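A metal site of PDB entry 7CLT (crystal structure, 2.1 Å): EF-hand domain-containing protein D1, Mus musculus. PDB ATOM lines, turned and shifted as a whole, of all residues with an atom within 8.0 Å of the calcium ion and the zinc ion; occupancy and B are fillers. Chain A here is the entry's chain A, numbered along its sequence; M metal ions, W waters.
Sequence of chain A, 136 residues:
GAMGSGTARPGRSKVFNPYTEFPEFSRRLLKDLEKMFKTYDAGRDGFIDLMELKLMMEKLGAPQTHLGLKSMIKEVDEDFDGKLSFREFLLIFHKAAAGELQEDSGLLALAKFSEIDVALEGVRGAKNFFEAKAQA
Within 4 Å of the zinc ion: Asp 79 and Asp 81.
The nearest printed residue that does not touch the zinc ion is Phe 47 (4.1 Å).
The side-chain carboxylate (OD2) of Asp 77 sits close to the backbone NH (N) of Phe 80 (3.2 Å).
The side-chain carboxylate (OD1) of Asp 77 sits at hydrogen-bond distance from the backbone NH (N) of Gly 82 (2.6 Å).
The side-chain carboxylate of Glu 88 lies close to the backbone NH of Ser 85, 3.1 Å away.
OE1 of Glu 88 sits close to N of Glu 78, 3.0 Å away.
The zinc ion is bound by the side-chain carboxylate (OD1) of Asp 81 (2.0 Å), the side-chain carboxylate (OD1) of Asp 79 (2.0 Å) and water W1 (2.2 Å).
The zinc ion has three donor atoms within binding distance.
The calcium ion is bound by OD2 of Asp 77, 2.3 Å away.
O of Lys 83 binds the calcium ion, 2.3 Å away.
OE2 of Glu 88 is bound to the calcium ion.
The calcium ion is bound by OD2 of Asp 79.
The calcium ion is bound by the side-chain carboxylate (OD2) of Asp 81.
OE1 of Glu 88 is bound to the calcium ion (2.6 Å).
Slightly farther from the calcium ion lies water W1 (2.9 Å).
Five residues have an atom within 4 Å of the calcium ion: Asp 77, Asp 79, Asp 81, Lys 83 and Glu 88.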
ATOM      1  N   GLY A  46       5.652 -15.014 -24.719  1.00  0.00           N
ATOM      2  CA  GLY A  46       4.643 -15.871 -25.319  1.00  0.00           C
ATOM      3  C   GLY A  46       3.322 -15.195 -25.626  1.00  0.00           C
ATOM      4  O   GLY A  46       2.357 -15.891 -26.004  1.00  0.00           O
ATOM      5  N   PHE A  47       3.232 -13.871 -25.471  1.00  0.00           N
ATOM      6  CA  PHE A  47       2.028 -13.100 -25.719  1.00  0.00           C
ATOM      7  C   PHE A  47       2.367 -11.905 -26.594  1.00  0.00           C
ATOM      8  O   PHE A  47       3.498 -11.412 -26.585  1.00  0.00           O
ATOM      9  CB  PHE A  47       1.395 -12.620 -24.405  1.00  0.00           C
ATOM     10  CG  PHE A  47       1.123 -13.728 -23.425  1.00  0.00           C
ATOM     11  CD1 PHE A  47       1.943 -13.902 -22.309  1.00  0.00           C
ATOM     12  CD2 PHE A  47       0.078 -14.625 -23.639  1.00  0.00           C
ATOM     13  CE1 PHE A  47       1.696 -14.930 -21.421  1.00  0.00           C
ATOM     14  CE2 PHE A  47      -0.176 -15.662 -22.738  1.00  0.00           C
ATOM     15  CZ  PHE A  47       0.651 -15.815 -21.627  1.00  0.00           C
ATOM     16  N   ILE A  48       1.395 -11.448 -27.369  1.00  0.00           N
ATOM     17  CA  ILE A  48       1.458 -10.127 -28.011  1.00  0.00           C
ATOM     18  C   ILE A  48       0.498  -9.235 -27.225  1.00  0.00           C
ATOM     19  O   ILE A  48      -0.722  -9.472 -27.203  1.00  0.00           O
ATOM     20  CB  ILE A  48       1.135 -10.192 -29.504  1.00  0.00           C
ATOM     21  CG1 ILE A  48       2.283 -10.903 -30.240  1.00  0.00           C
ATOM     22  CG2 ILE A  48       0.926  -8.761 -30.078  1.00  0.00           C
ATOM     23  CD1 ILE A  48       2.073 -11.112 -31.711  1.00  0.00           C
ATOM     24  N   ILE A  73      -8.032  -6.863 -29.983  1.00  0.00           N
ATOM     25  CA  ILE A  73      -7.674  -7.929 -29.050  1.00  0.00           C
ATOM     26  C   ILE A  73      -8.928  -8.586 -28.483  1.00  0.00           C
ATOM     27  O   ILE A  73      -9.056  -9.815 -28.467  1.00  0.00           O
ATOM     28  CB  ILE A  73      -6.752  -7.386 -27.939  1.00  0.00           C
ATOM     29  CG1 ILE A  73      -5.365  -7.068 -28.524  1.00  0.00           C
ATOM     30  CG2 ILE A  73      -6.622  -8.443 -26.798  1.00  0.00           C
ATOM     31  CD1 ILE A  73      -4.454  -6.414 -27.542  1.00  0.00           C
ATOM     32  N   VAL A  76     -10.754 -11.654 -30.151  1.00  0.00           N
ATOM     33  CA  VAL A  76     -10.223 -13.006 -30.112  1.00  0.00           C
ATOM     34  C   VAL A  76      -9.623 -13.303 -28.754  1.00  0.00           C
ATOM     35  O   VAL A  76      -8.947 -14.321 -28.579  1.00  0.00           O
ATOM     36  CB  VAL A  76      -9.156 -13.254 -31.214  1.00  0.00           C
ATOM     37  CG1 VAL A  76      -9.785 -13.291 -32.597  1.00  0.00           C
ATOM     38  CG2 VAL A  76      -8.023 -12.217 -31.138  1.00  0.00           C
ATOM     39  N   ASP A  77      -9.848 -12.427 -27.767  1.00  0.00           N
ATOM     40  CA  ASP A  77      -9.233 -12.596 -26.435  1.00  0.00           C
ATOM     41  C   ASP A  77     -10.116 -13.547 -25.613  1.00  0.00           C
ATOM     42  O   ASP A  77     -10.846 -13.142 -24.705  1.00  0.00           O
ATOM     43  CB  ASP A  77      -9.069 -11.240 -25.749  1.00  0.00           C
ATOM     44  CG  ASP A  77      -8.351 -11.335 -24.402  1.00  0.00           C
ATOM     45  OD1 ASP A  77      -8.447 -10.375 -23.618  1.00  0.00           O
ATOM     46  OD2 ASP A  77      -7.708 -12.356 -24.123  1.00  0.00           O
ATOM     47  N   GLU A  78     -10.034 -14.842 -25.938  1.00  0.00           N
ATOM     48  CA  GLU A  78     -10.969 -15.820 -25.386  1.00  0.00           C
ATOM     49  C   GLU A  78     -10.821 -16.002 -23.884  1.00  0.00           C
ATOM     50  O   GLU A  78     -11.767 -16.466 -23.248  1.00  0.00           O
ATOM     51  CB  GLU A  78     -10.800 -17.175 -26.085  1.00  0.00           C
ATOM     52  CG  GLU A  78     -11.206 -17.172 -27.559  1.00  0.00           C
ATOM     53  CD  GLU A  78     -10.929 -18.494 -28.245  1.00  0.00           C
ATOM     54  OE1 GLU A  78     -10.015 -19.222 -27.807  1.00  0.00           O
ATOM     55  OE2 GLU A  78     -11.618 -18.813 -29.227  1.00  0.00           O
ATOM     56  N   ASP A  79      -9.667 -15.676 -23.294  1.00  0.00           N
ATOM     57  CA  ASP A  79      -9.509 -15.784 -21.849  1.00  0.00           C
ATOM     58  C   ASP A  79      -9.468 -14.416 -21.152  1.00  0.00           C
ATOM     59  O   ASP A  79      -9.105 -14.350 -19.976  1.00  0.00           O
ATOM     60  CB  ASP A  79      -8.268 -16.608 -21.495  1.00  0.00           C
ATOM     61  CG  ASP A  79      -6.983 -15.959 -21.896  1.00  0.00           C
ATOM     62  OD1 ASP A  79      -5.927 -16.516 -21.547  1.00  0.00           O
ATOM     63  OD2 ASP A  79      -7.000 -14.909 -22.571  1.00  0.00           O
ATOM     64  N   PHE A  80      -9.800 -13.349 -21.856  1.00  0.00           N
ATOM     65  CA  PHE A  80     -10.175 -12.070 -21.252  1.00  0.00           C
ATOM     66  C   PHE A  80      -9.037 -11.401 -20.476  1.00  0.00           C
ATOM     67  O   PHE A  80      -9.287 -10.636 -19.542  1.00  0.00           O
ATOM     68  CB  PHE A  80     -11.411 -12.243 -20.352  1.00  0.00           C
ATOM     69  CG  PHE A  80     -12.594 -12.813 -21.075  1.00  0.00           C
ATOM     70  CD1 PHE A  80     -12.831 -14.185 -21.071  1.00  0.00           C
ATOM     71  CD2 PHE A  80     -13.454 -12.001 -21.787  1.00  0.00           C
ATOM     72  CE1 PHE A  80     -13.903 -14.718 -21.740  1.00  0.00           C
ATOM     73  CE2 PHE A  80     -14.543 -12.534 -22.457  1.00  0.00           C
ATOM     74  CZ  PHE A  80     -14.759 -13.899 -22.436  1.00  0.00           C
ATOM     75  N   ASP A  81      -7.770 -11.631 -20.840  1.00  0.00           N
ATOM     76  CA  ASP A  81      -6.684 -10.977 -20.133  1.00  0.00           C
ATOM     77  C   ASP A  81      -6.041  -9.837 -20.914  1.00  0.00           C
ATOM     78  O   ASP A  81      -5.011  -9.304 -20.477  1.00  0.00           O
ATOM     79  CB  ASP A  81      -5.605 -11.989 -19.729  1.00  0.00           C
ATOM     80  CG  ASP A  81      -5.114 -12.807 -20.894  1.00  0.00           C
ATOM     81  OD1 ASP A  81      -4.450 -13.837 -20.650  1.00  0.00           O
ATOM     82  OD2 ASP A  81      -5.396 -12.453 -22.055  1.00  0.00           O
ATOM     83  N   GLY A  82      -6.591  -9.444 -22.054  1.00  0.00           N
ATOM     84  CA  GLY A  82      -6.078  -8.274 -22.737  1.00  0.00           C
ATOM     85  C   GLY A  82      -4.801  -8.477 -23.532  1.00  0.00           C
ATOM     86  O   GLY A  82      -4.232  -7.497 -24.017  1.00  0.00           O
ATOM     87  N   LYS A  83      -4.324  -9.707 -23.667  1.00  0.00           N
ATOM     88  CA  LYS A  83      -3.155  -9.977 -24.498  1.00  0.00           C
ATOM     89  C   LYS A  83      -3.438 -11.218 -25.329  1.00  0.00           C
ATOM     90  O   LYS A  83      -4.338 -12.002 -25.024  1.00  0.00           O
ATOM     91  CB  LYS A  83      -1.887 -10.185 -23.650  1.00  0.00           C
ATOM     92  CG  LYS A  83      -1.923 -11.443 -22.794  1.00  0.00           C
ATOM     93  CD  LYS A  83      -0.956 -11.273 -21.620  1.00  0.00           C
ATOM     94  CE  LYS A  83      -0.985 -12.470 -20.703  1.00  0.00           C
ATOM     95  NZ  LYS A  83       0.101 -12.398 -19.702  1.00  0.00           N
ATOM     96  N   LEU A  84      -2.658 -11.392 -26.388  1.00  0.00           N
ATOM     97  CA  LEU A  84      -2.906 -12.455 -27.353  1.00  0.00           C
ATOM     98  C   LEU A  84      -1.890 -13.567 -27.160  1.00  0.00           C
ATOM     99  O   LEU A  84      -0.682 -13.345 -27.362  1.00  0.00           O
ATOM    100  CB  LEU A  84      -2.827 -11.938 -28.776  1.00  0.00           C
ATOM    101  CG  LEU A  84      -3.817 -10.852 -29.195  1.00  0.00           C
ATOM    102  CD1 LEU A  84      -3.413 -10.314 -30.559  1.00  0.00           C
ATOM    103  CD2 LEU A  84      -5.228 -11.396 -29.190  1.00  0.00           C
ATOM    104  N   SER A  85      -2.362 -14.748 -26.787  1.00  0.00           N
ATOM    105  CA  SER A  85      -1.554 -15.948 -26.861  1.00  0.00           C
ATOM    106  C   SER A  85      -1.482 -16.394 -28.324  1.00  0.00           C
ATOM    107  O   SER A  85      -2.185 -15.858 -29.183  1.00  0.00           O
ATOM    108  CB  SER A  85      -2.150 -17.051 -25.967  1.00  0.00           C
ATOM    109  OG  SER A  85      -3.422 -17.490 -26.462  1.00  0.00           O
ATOM    110  N   PHE A  86      -0.625 -17.379 -28.613  1.00  0.00           N
ATOM    111  CA  PHE A  86      -0.454 -17.805 -30.008  1.00  0.00           C
ATOM    112  C   PHE A  86      -1.715 -18.453 -30.574  1.00  0.00           C
ATOM    113  O   PHE A  86      -2.006 -18.321 -31.772  1.00  0.00           O
ATOM    114  CB  PHE A  86       0.732 -18.746 -30.144  1.00  0.00           C
ATOM    115  CG  PHE A  86       0.939 -19.270 -31.557  1.00  0.00           C
ATOM    116  CD1 PHE A  86       1.284 -18.404 -32.576  1.00  0.00           C
ATOM    117  CD2 PHE A  86       0.781 -20.608 -31.850  1.00  0.00           C
ATOM    118  CE1 PHE A  86       1.464 -18.861 -33.886  1.00  0.00           C
ATOM    119  CE2 PHE A  86       0.978 -21.078 -33.153  1.00  0.00           C
ATOM    120  CZ  PHE A  86       1.323 -20.188 -34.170  1.00  0.00           C
ATOM    121  N   ARG A  87      -2.487 -19.174 -29.754  1.00  0.00           N
ATOM    122  CA  ARG A  87      -3.722 -19.733 -30.297  1.00  0.00           C
ATOM    123  C   ARG A  87      -4.736 -18.640 -30.640  1.00  0.00           C
ATOM    124  O   ARG A  87      -5.500 -18.770 -31.615  1.00  0.00           O
ATOM    125  CB  ARG A  87      -4.323 -20.743 -29.326  1.00  0.00           C
ATOM    126  CG  ARG A  87      -4.700 -20.180 -27.961  1.00  0.00           C
ATOM    127  CD  ARG A  87      -5.148 -21.294 -27.026  1.00  0.00           C
ATOM    128  NE  ARG A  87      -6.338 -21.973 -27.552  1.00  0.00           N
ATOM    129  CZ  ARG A  87      -6.712 -23.186 -27.186  1.00  0.00           C
ATOM    130  NH1 ARG A  87      -7.808 -23.745 -27.716  1.00  0.00           N
ATOM    131  NH2 ARG A  87      -6.001 -23.856 -26.293  1.00  0.00           N
ATOM    132  N   GLU A  88      -4.774 -17.561 -29.849  1.00  0.00           N
ATOM    133  CA  GLU A  88      -5.656 -16.439 -30.186  1.00  0.00           C
ATOM    134  C   GLU A  88      -5.180 -15.733 -31.438  1.00  0.00           C
ATOM    135  O   GLU A  88      -5.987 -15.242 -32.239  1.00  0.00           O
ATOM    136  CB  GLU A  88      -5.730 -15.461 -29.007  1.00  0.00           C
ATOM    137  CG  GLU A  88      -6.350 -16.078 -27.747  1.00  0.00           C
ATOM    138  CD  GLU A  88      -6.265 -15.180 -26.538  1.00  0.00           C
ATOM    139  OE1 GLU A  88      -7.090 -15.360 -25.629  1.00  0.00           O
ATOM    140  OE2 GLU A  88      -5.380 -14.286 -26.473  1.00  0.00           O
ATOM    141  N   PHE A  89      -3.870 -15.635 -31.626  1.00  0.00           N
ATOM    142  CA  PHE A  89      -3.348 -14.982 -32.821  1.00  0.00           C
ATOM    143  C   PHE A  89      -3.690 -15.779 -34.075  1.00  0.00           C
ATOM    144  O   PHE A  89      -4.064 -15.206 -35.101  1.00  0.00           O
ATOM    145  CB  PHE A  89      -1.827 -14.786 -32.641  1.00  0.00           C
ATOM    146  CG  PHE A  89      -1.127 -14.211 -33.819  1.00  0.00           C
ATOM    147  CD1 PHE A  89      -1.109 -12.842 -34.028  1.00  0.00           C
ATOM    148  CD2 PHE A  89      -0.447 -15.028 -34.704  1.00  0.00           C
ATOM    149  CE1 PHE A  89      -0.440 -12.294 -35.117  1.00  0.00           C
ATOM    150  CE2 PHE A  89       0.228 -14.483 -35.800  1.00  0.00           C
ATOM    151  CZ  PHE A  89       0.222 -13.111 -36.004  1.00  0.00           C
HETATM  152 CA    CA M   1      -5.813 -13.580 -24.222  1.00  0.00          CA
HETATM  153 ZN    ZN M   2      -4.174 -15.546 -21.662  1.00  0.00          ZN
HETATM  154  O   HOH W   1      -3.429 -15.225 -23.664  1.00  0.00           O
